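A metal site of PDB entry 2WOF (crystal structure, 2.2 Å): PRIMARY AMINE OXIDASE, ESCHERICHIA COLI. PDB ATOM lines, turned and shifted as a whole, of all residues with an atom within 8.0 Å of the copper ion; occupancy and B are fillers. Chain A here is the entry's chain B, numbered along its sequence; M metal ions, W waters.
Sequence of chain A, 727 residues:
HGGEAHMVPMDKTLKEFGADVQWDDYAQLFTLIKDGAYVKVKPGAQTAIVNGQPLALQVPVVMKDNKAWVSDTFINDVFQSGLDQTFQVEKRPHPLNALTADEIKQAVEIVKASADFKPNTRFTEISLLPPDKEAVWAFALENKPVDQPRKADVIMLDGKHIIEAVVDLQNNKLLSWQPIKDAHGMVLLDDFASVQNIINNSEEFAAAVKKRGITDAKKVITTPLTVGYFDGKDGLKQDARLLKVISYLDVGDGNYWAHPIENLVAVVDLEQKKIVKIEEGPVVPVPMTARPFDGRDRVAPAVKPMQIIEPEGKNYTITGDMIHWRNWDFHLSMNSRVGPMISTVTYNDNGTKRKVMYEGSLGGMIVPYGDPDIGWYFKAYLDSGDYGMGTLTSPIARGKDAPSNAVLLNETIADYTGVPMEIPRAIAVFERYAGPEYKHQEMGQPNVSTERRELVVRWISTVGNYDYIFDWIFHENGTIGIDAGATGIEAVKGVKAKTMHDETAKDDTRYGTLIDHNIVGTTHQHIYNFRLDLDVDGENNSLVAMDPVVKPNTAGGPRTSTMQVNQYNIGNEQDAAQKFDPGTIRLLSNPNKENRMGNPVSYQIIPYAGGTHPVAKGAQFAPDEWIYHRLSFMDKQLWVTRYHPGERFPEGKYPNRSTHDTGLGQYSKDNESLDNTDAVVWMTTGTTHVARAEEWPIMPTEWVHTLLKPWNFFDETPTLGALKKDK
The backbone carbonyl oxygen of His 526 lies within hydrogen-bond range of the backbone NH of Thr 687.
A ring nitrogen (NE2) of His 689 lies within hydrogen-bond range of the side-chain carboxylate (OE1) of Glu 695, 2.6 Å away.
A ring nitrogen (ND1) of His 524 sits at hydrogen-bond distance from the backbone carbonyl oxygen (O) of Thr 522, 2.8 Å away.
The side-chain hydroxyl (OH) of Tyr 468 lies within hydrogen-bond range of a ring nitrogen (ND1) of His 526.
Along chain A the residues within 4 Å of the copper ion span positions 524 to 689.
The nearest printed residue that does not touch the copper ion is TPQ 466 (4.8 Å).
The copper ion is bound by a ring nitrogen (NE2) of His 526, 2.1 Å away.
NE2 of His 524 binds the copper ion (2.1 Å).
The copper ion is bound by ND1 of His 689 (2.2 Å).
The copper ion has three donor atoms within binding distance.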
ATOM      1  N   VAL A 367      -5.441  31.839 -23.275  1.00  0.00           N
ATOM      2  CA  VAL A 367      -6.349  30.904 -23.915  1.00  0.00           C
ATOM      3  C   VAL A 367      -7.693  31.580 -24.115  1.00  0.00           C
ATOM      4  O   VAL A 367      -8.572  31.472 -23.256  1.00  0.00           O
ATOM      5  CB  VAL A 367      -6.570  29.681 -23.066  1.00  0.00           C
ATOM      6  CG1 VAL A 367      -7.422  28.630 -23.840  1.00  0.00           C
ATOM      7  CG2 VAL A 367      -5.227  29.087 -22.679  1.00  0.00           C
ATOM      8  N   TYR A 369     -11.306  32.517 -26.207  1.00  0.00           N
ATOM      9  CA  TYR A 369     -12.333  31.812 -26.928  1.00  0.00           C
ATOM     10  C   TYR A 369     -12.980  32.703 -27.972  1.00  0.00           C
ATOM     11  O   TYR A 369     -12.661  33.923 -28.087  1.00  0.00           O
ATOM     12  CB  TYR A 369     -13.349  31.237 -25.982  1.00  0.00           C
ATOM     13  CG  TYR A 369     -12.857  29.999 -25.225  1.00  0.00           C
ATOM     14  CD1 TYR A 369     -11.954  30.114 -24.175  1.00  0.00           C
ATOM     15  CD2 TYR A 369     -13.293  28.721 -25.554  1.00  0.00           C
ATOM     16  CE1 TYR A 369     -11.471  29.004 -23.527  1.00  0.00           C
ATOM     17  CE2 TYR A 369     -12.860  27.609 -24.899  1.00  0.00           C
ATOM     18  CZ  TYR A 369     -11.914  27.765 -23.871  1.00  0.00           C
ATOM     19  OH  TYR A 369     -11.491  26.674 -23.186  1.00  0.00           O
ATOM     20  N   ASN A 465      -9.972  23.184 -16.038  1.00  0.00           N
ATOM     21  CA  ASN A 465     -10.126  21.992 -16.882  1.00  0.00           C
ATOM     22  C   ASN A 465      -8.848  21.668 -17.711  1.00  0.00           C
ATOM     23  O   ASN A 465      -8.720  20.556 -18.213  1.00  0.00           O
ATOM     24  CB  ASN A 465     -11.312  22.135 -17.825  1.00  0.00           C
ATOM     25  CG  ASN A 465     -11.230  23.375 -18.619  1.00  0.00           C
ATOM     26  OD1 ASN A 465     -10.948  24.442 -18.083  1.00  0.00           O
ATOM     27  ND2 ASN A 465     -11.387  23.253 -19.920  1.00  0.00           N
ATOM     28  N   TPQ A 466      -7.935  22.484 -17.927  1.00  0.00           N
ATOM     29  CA  TPQ A 466      -6.738  22.273 -18.766  1.00  0.00           C
ATOM     30  CB  TPQ A 466      -6.209  23.540 -19.439  1.00  0.00           C
ATOM     31  C   TPQ A 466      -5.537  21.832 -17.971  1.00  0.00           C
ATOM     32  O   TPQ A 466      -5.142  22.493 -16.983  1.00  0.00           O
ATOM     33  C1  TPQ A 466      -7.318  24.449 -19.876  1.00  0.00           C
ATOM     34  C2  TPQ A 466      -8.083  24.137 -21.125  1.00  0.00           C
ATOM     35  O2  TPQ A 466      -7.785  23.002 -21.847  1.00  0.00           O
ATOM     36  C3  TPQ A 466      -9.121  24.989 -21.518  1.00  0.00           C
ATOM     37  C4  TPQ A 466      -9.393  26.136 -20.746  1.00  0.00           C
ATOM     38  O4  TPQ A 466     -10.379  26.996 -21.089  1.00  0.00           O
ATOM     39  C5  TPQ A 466      -8.606  26.418 -19.509  1.00  0.00           C
ATOM     40  O5  TPQ A 466      -8.889  27.510 -18.750  1.00  0.00           O
ATOM     41  C6  TPQ A 466      -7.587  25.576 -19.113  1.00  0.00           C
ATOM     42  N   TYR A 468      -1.282  21.731 -18.550  1.00  0.00           N
ATOM     43  CA  TYR A 468      -0.211  22.162 -19.457  1.00  0.00           C
ATOM     44  C   TYR A 468       1.067  21.568 -19.062  1.00  0.00           C
ATOM     45  O   TYR A 468       1.405  21.593 -17.902  1.00  0.00           O
ATOM     46  CB  TYR A 468      -0.138  23.676 -19.459  1.00  0.00           C
ATOM     47  CG  TYR A 468      -1.399  24.312 -20.031  1.00  0.00           C
ATOM     48  CD1 TYR A 468      -1.657  24.242 -21.391  1.00  0.00           C
ATOM     49  CD2 TYR A 468      -2.342  24.911 -19.221  1.00  0.00           C
ATOM     50  CE1 TYR A 468      -2.799  24.778 -21.946  1.00  0.00           C
ATOM     51  CE2 TYR A 468      -3.472  25.469 -19.744  1.00  0.00           C
ATOM     52  CZ  TYR A 468      -3.703  25.390 -21.129  1.00  0.00           C
ATOM     53  OH  TYR A 468      -4.857  25.907 -21.725  1.00  0.00           O
ATOM     54  N   ALA A 486      -0.568  20.501 -24.192  1.00  0.00           N
ATOM     55  CA  ALA A 486      -1.893  20.809 -23.645  1.00  0.00           C
ATOM     56  C   ALA A 486      -2.742  19.497 -23.649  1.00  0.00           C
ATOM     57  O   ALA A 486      -2.784  18.756 -24.621  1.00  0.00           O
ATOM     58  CB  ALA A 486      -2.562  21.874 -24.506  1.00  0.00           C
ATOM     59  N   THR A 487      -3.364  19.217 -22.525  1.00  0.00           N
ATOM     60  CA  THR A 487      -4.294  18.080 -22.425  1.00  0.00           C
ATOM     61  C   THR A 487      -5.356  18.538 -21.387  1.00  0.00           C
ATOM     62  O   THR A 487      -5.451  19.741 -21.051  1.00  0.00           O
ATOM     63  CB  THR A 487      -3.543  16.743 -22.090  1.00  0.00           C
ATOM     64  OG1 THR A 487      -4.469  15.661 -21.923  1.00  0.00           O
ATOM     65  CG2 THR A 487      -2.707  16.888 -20.812  1.00  0.00           C
ATOM     66  N   ILE A 489      -9.497  18.508 -20.020  1.00  0.00           N
ATOM     67  CA  ILE A 489     -10.898  18.400 -20.406  1.00  0.00           C
ATOM     68  C   ILE A 489     -11.347  19.670 -21.093  1.00  0.00           C
ATOM     69  O   ILE A 489     -11.129  20.749 -20.609  1.00  0.00           O
ATOM     70  CB  ILE A 489     -11.821  18.152 -19.207  1.00  0.00           C
ATOM     71  CG1 ILE A 489     -11.250  17.096 -18.292  1.00  0.00           C
ATOM     72  CG2 ILE A 489     -13.265  17.654 -19.686  1.00  0.00           C
ATOM     73  CD1 ILE A 489     -10.982  15.783 -18.950  1.00  0.00           C
ATOM     74  N   GLU A 490     -11.959  19.555 -22.250  1.00  0.00           N
ATOM     75  CA  GLU A 490     -12.419  20.723 -22.969  1.00  0.00           C
ATOM     76  C   GLU A 490     -13.513  21.539 -22.270  1.00  0.00           C
ATOM     77  O   GLU A 490     -14.401  20.971 -21.663  1.00  0.00           O
ATOM     78  CB  GLU A 490     -12.936  20.284 -24.358  1.00  0.00           C
ATOM     79  CG  GLU A 490     -11.830  20.065 -25.281  1.00  0.00           C
ATOM     80  CD  GLU A 490     -12.158  20.571 -26.637  1.00  0.00           C
ATOM     81  OE1 GLU A 490     -12.308  21.827 -26.814  1.00  0.00           O
ATOM     82  OE2 GLU A 490     -12.245  19.682 -27.523  1.00  0.00           O
ATOM     83  N   ALA A 491     -13.473  22.848 -22.415  1.00  0.00           N
ATOM     84  CA  ALA A 491     -14.605  23.709 -22.068  1.00  0.00           C
ATOM     85  C   ALA A 491     -15.667  23.557 -23.164  1.00  0.00           C
ATOM     86  O   ALA A 491     -15.412  23.883 -24.341  1.00  0.00           O
ATOM     87  CB  ALA A 491     -14.177  25.107 -21.994  1.00  0.00           C
ATOM     88  N   THR A 522     -16.138  24.485 -27.984  1.00  0.00           N
ATOM     89  CA  THR A 522     -15.989  25.780 -28.522  1.00  0.00           C
ATOM     90  C   THR A 522     -14.549  26.073 -28.969  1.00  0.00           C
ATOM     91  O   THR A 522     -13.588  25.833 -28.242  1.00  0.00           O
ATOM     92  CB  THR A 522     -16.430  26.830 -27.527  1.00  0.00           C
ATOM     93  OG1 THR A 522     -17.734  26.485 -27.019  1.00  0.00           O
ATOM     94  CG2 THR A 522     -16.480  28.164 -28.211  1.00  0.00           C
ATOM     95  N   THR A 523     -14.418  26.597 -30.187  1.00  0.00           N
ATOM     96  CA  THR A 523     -13.139  26.978 -30.768  1.00  0.00           C
ATOM     97  C   THR A 523     -12.395  28.010 -29.920  1.00  0.00           C
ATOM     98  O   THR A 523     -13.019  28.949 -29.363  1.00  0.00           O
ATOM     99  CB  THR A 523     -13.337  27.501 -32.220  1.00  0.00           C
ATOM    100  OG1 THR A 523     -13.931  26.456 -33.012  1.00  0.00           O
ATOM    101  CG2 THR A 523     -12.038  27.920 -32.860  1.00  0.00           C
ATOM    102  N   HIS A 524     -11.084  27.846 -29.786  1.00  0.00           N
ATOM    103  CA  HIS A 524     -10.270  28.798 -29.001  1.00  0.00           C
ATOM    104  C   HIS A 524      -8.816  28.716 -29.402  1.00  0.00           C
ATOM    105  O   HIS A 524      -8.462  27.915 -30.196  1.00  0.00           O
ATOM    106  CB  HIS A 524     -10.432  28.463 -27.519  1.00  0.00           C
ATOM    107  CG  HIS A 524     -10.051  27.073 -27.192  1.00  0.00           C
ATOM    108  ND1 HIS A 524     -10.859  25.990 -27.466  1.00  0.00           N
ATOM    109  CD2 HIS A 524      -8.912  26.565 -26.680  1.00  0.00           C
ATOM    110  CE1 HIS A 524     -10.233  24.886 -27.125  1.00  0.00           C
ATOM    111  NE2 HIS A 524      -9.051  25.204 -26.660  1.00  0.00           N
ATOM    112  N   GLN A 525      -7.954  29.570 -28.843  1.00  0.00           N
ATOM    113  CA  GLN A 525      -6.533  29.471 -29.067  1.00  0.00           C
ATOM    114  C   GLN A 525      -5.751  29.190 -27.810  1.00  0.00           C
ATOM    115  O   GLN A 525      -6.204  29.513 -26.725  1.00  0.00           O
ATOM    116  CB  GLN A 525      -6.042  30.758 -29.625  1.00  0.00           C
ATOM    117  CG  GLN A 525      -6.376  30.919 -31.085  1.00  0.00           C
ATOM    118  CD  GLN A 525      -5.891  32.206 -31.622  1.00  0.00           C
ATOM    119  OE1 GLN A 525      -6.245  33.258 -31.101  1.00  0.00           O
ATOM    120  NE2 GLN A 525      -5.055  32.144 -32.664  1.00  0.00           N
ATOM    121  N   HIS A 526      -4.582  28.594 -27.955  1.00  0.00           N
ATOM    122  CA  HIS A 526      -3.650  28.499 -26.884  1.00  0.00           C
ATOM    123  C   HIS A 526      -2.409  29.246 -27.299  1.00  0.00           C
ATOM    124  O   HIS A 526      -1.771  28.902 -28.275  1.00  0.00           O
ATOM    125  CB  HIS A 526      -3.236  27.055 -26.589  1.00  0.00           C
ATOM    126  CG  HIS A 526      -4.328  26.162 -26.120  1.00  0.00           C
ATOM    127  ND1 HIS A 526      -4.739  26.113 -24.810  1.00  0.00           N
ATOM    128  CD2 HIS A 526      -5.079  25.265 -26.790  1.00  0.00           C
ATOM    129  CE1 HIS A 526      -5.700  25.208 -24.689  1.00  0.00           C
ATOM    130  NE2 HIS A 526      -5.924  24.690 -25.880  1.00  0.00           N
ATOM    131  N   TYR A 528       1.153  30.580 -25.936  1.00  0.00           N
ATOM    132  CA  TYR A 528       2.218  30.560 -24.934  1.00  0.00           C
ATOM    133  C   TYR A 528       3.271  31.541 -25.302  1.00  0.00           C
ATOM    134  O   TYR A 528       3.518  31.738 -26.469  1.00  0.00           O
ATOM    135  CB  TYR A 528       2.895  29.182 -24.904  1.00  0.00           C
ATOM    136  CG  TYR A 528       1.936  28.059 -24.897  1.00  0.00           C
ATOM    137  CD1 TYR A 528       1.410  27.578 -23.713  1.00  0.00           C
ATOM    138  CD2 TYR A 528       1.534  27.467 -26.074  1.00  0.00           C
ATOM    139  CE1 TYR A 528       0.498  26.478 -23.705  1.00  0.00           C
ATOM    140  CE2 TYR A 528       0.618  26.386 -26.091  1.00  0.00           C
ATOM    141  CZ  TYR A 528       0.111  25.895 -24.910  1.00  0.00           C
ATOM    142  OH  TYR A 528      -0.796  24.865 -24.905  1.00  0.00           O
ATOM    143  N   HIS A 613      -1.503  20.595 -33.518  1.00  0.00           N
ATOM    144  CA  HIS A 613      -2.797  21.244 -33.781  1.00  0.00           C
ATOM    145  C   HIS A 613      -2.509  22.312 -34.878  1.00  0.00           C
ATOM    146  O   HIS A 613      -1.357  22.728 -35.091  1.00  0.00           O
ATOM    147  CB  HIS A 613      -3.299  21.993 -32.538  1.00  0.00           C
ATOM    148  CG  HIS A 613      -4.291  21.245 -31.708  1.00  0.00           C
ATOM    149  ND1 HIS A 613      -5.097  20.255 -32.214  1.00  0.00           N
ATOM    150  CD2 HIS A 613      -4.658  21.407 -30.415  1.00  0.00           C
ATOM    151  CE1 HIS A 613      -5.874  19.775 -31.248  1.00  0.00           C
ATOM    152  NE2 HIS A 613      -5.646  20.489 -30.148  1.00  0.00           N
ATOM    153  N   THR A 687      -1.645  27.558 -30.772  1.00  0.00           N
ATOM    154  CA  THR A 687      -2.467  26.734 -31.633  1.00  0.00           C
ATOM    155  C   THR A 687      -3.816  27.420 -31.796  1.00  0.00           C
ATOM    156  O   THR A 687      -4.211  28.274 -30.981  1.00  0.00           O
ATOM    157  CB  THR A 687      -2.673  25.348 -31.006  1.00  0.00           C
ATOM    158  OG1 THR A 687      -3.394  25.469 -29.791  1.00  0.00           O
ATOM    159  CG2 THR A 687      -1.356  24.703 -30.707  1.00  0.00           C
ATOM    160  N   THR A 688      -4.503  27.076 -32.880  1.00  0.00           N
ATOM    161  CA  THR A 688      -5.919  27.338 -33.032  1.00  0.00           C
ATOM    162  C   THR A 688      -6.604  25.996 -32.910  1.00  0.00           C
ATOM    163  O   THR A 688      -6.434  25.091 -33.725  1.00  0.00           O
ATOM    164  CB  THR A 688      -6.239  28.013 -34.403  1.00  0.00           C
ATOM    165  OG1 THR A 688      -5.758  29.358 -34.391  1.00  0.00           O
ATOM    166  CG2 THR A 688      -7.746  28.060 -34.651  1.00  0.00           C
ATOM    167  N   HIS A 689      -7.380  25.831 -31.842  1.00  0.00           N
ATOM    168  CA  HIS A 689      -7.927  24.556 -31.554  1.00  0.00           C
ATOM    169  C   HIS A 689      -9.405  24.433 -32.016  1.00  0.00           C
ATOM    170  O   HIS A 689     -10.294  24.951 -31.368  1.00  0.00           O
ATOM    171  CB  HIS A 689      -7.758  24.257 -30.030  1.00  0.00           C
ATOM    172  CG  HIS A 689      -8.306  22.919 -29.617  1.00  0.00           C
ATOM    173  ND1 HIS A 689      -8.280  22.457 -28.321  1.00  0.00           N
ATOM    174  CD2 HIS A 689      -8.881  21.934 -30.360  1.00  0.00           C
ATOM    175  CE1 HIS A 689      -8.836  21.252 -28.265  1.00  0.00           C
ATOM    176  NE2 HIS A 689      -9.201  20.918 -29.493  1.00  0.00           N
ATOM    177  N   VAL A 690      -9.619  23.713 -33.107  1.00  0.00           N
ATOM    178  CA  VAL A 690     -10.962  23.293 -33.558  1.00  0.00           C
ATOM    179  C   VAL A 690     -11.114  21.842 -33.164  1.00  0.00           C
ATOM    180  O   VAL A 690     -10.298  20.984 -33.524  1.00  0.00           O
ATOM    181  CB  VAL A 690     -11.143  23.442 -35.093  1.00  0.00           C
ATOM    182  CG1 VAL A 690     -12.506  22.913 -35.570  1.00  0.00           C
ATOM    183  CG2 VAL A 690     -10.984  24.857 -35.514  1.00  0.00           C
ATOM    184  N   ALA A 691     -12.177  21.560 -32.421  1.00  0.00           N
ATOM    185  CA  ALA A 691     -12.271  20.342 -31.673  1.00  0.00           C
ATOM    186  C   ALA A 691     -12.705  19.154 -32.529  1.00  0.00           C
ATOM    187  O   ALA A 691     -13.102  19.316 -33.644  1.00  0.00           O
ATOM    188  CB  ALA A 691     -13.214  20.545 -30.423  1.00  0.00           C
ATOM    189  N   GLU A 695     -11.308  14.034 -29.068  1.00  0.00           N
ATOM    190  CA  GLU A 695     -10.823  14.805 -27.887  1.00  0.00           C
ATOM    191  C   GLU A 695     -11.762  14.831 -26.647  1.00  0.00           C
ATOM    192  O   GLU A 695     -11.562  15.656 -25.718  1.00  0.00           O
ATOM    193  CB  GLU A 695     -10.489  16.236 -28.314  1.00  0.00           C
ATOM    194  CG  GLU A 695      -9.473  16.276 -29.468  1.00  0.00           C
ATOM    195  CD  GLU A 695      -9.320  17.651 -30.135  1.00  0.00           C
ATOM    196  OE1 GLU A 695     -10.204  18.523 -29.978  1.00  0.00           O
ATOM    197  OE2 GLU A 695      -8.347  17.830 -30.893  1.00  0.00           O
ATOM    198  N   MET A 699      -8.811  14.887 -23.639  1.00  0.00           N
ATOM    199  CA  MET A 699      -8.052  15.302 -24.808  1.00  0.00           C
ATOM    200  C   MET A 699      -6.637  14.731 -24.810  1.00  0.00           C
ATOM    201  O   MET A 699      -5.889  14.874 -23.863  1.00  0.00           O
ATOM    202  CB  MET A 699      -7.991  16.841 -24.897  1.00  0.00           C
ATOM    203  CG  MET A 699      -6.650  17.384 -25.569  1.00  0.00           C
ATOM    204  SD  MET A 699      -6.639  18.883 -26.691  1.00  0.00           S
ATOM    205  CE  MET A 699      -5.040  19.575 -26.241  1.00  0.00           C
ATOM    206  N   GLU A 702      -1.546  17.384 -26.978  1.00  0.00           N
ATOM    207  CA  GLU A 702      -1.112  18.034 -28.204  1.00  0.00           C
ATOM    208  C   GLU A 702       0.146  18.937 -27.909  1.00  0.00           C
ATOM    209  O   GLU A 702       0.217  19.626 -26.881  1.00  0.00           O
ATOM    210  CB  GLU A 702      -2.264  18.915 -28.720  1.00  0.00           C
ATOM    211  CG  GLU A 702      -3.510  18.188 -29.135  1.00  0.00           C
ATOM    212  CD  GLU A 702      -3.401  17.423 -30.459  1.00  0.00           C
ATOM    213  OE1 GLU A 702      -2.312  17.426 -31.114  1.00  0.00           O
ATOM    214  OE2 GLU A 702      -4.435  16.828 -30.840  1.00  0.00           O
HETATM  215 CU    CU M   1      -7.594  23.677 -26.590  1.00  0.00          CU
HETATM  216  O   HOH W   1      -8.951  22.911 -23.967  1.00  0.00           O
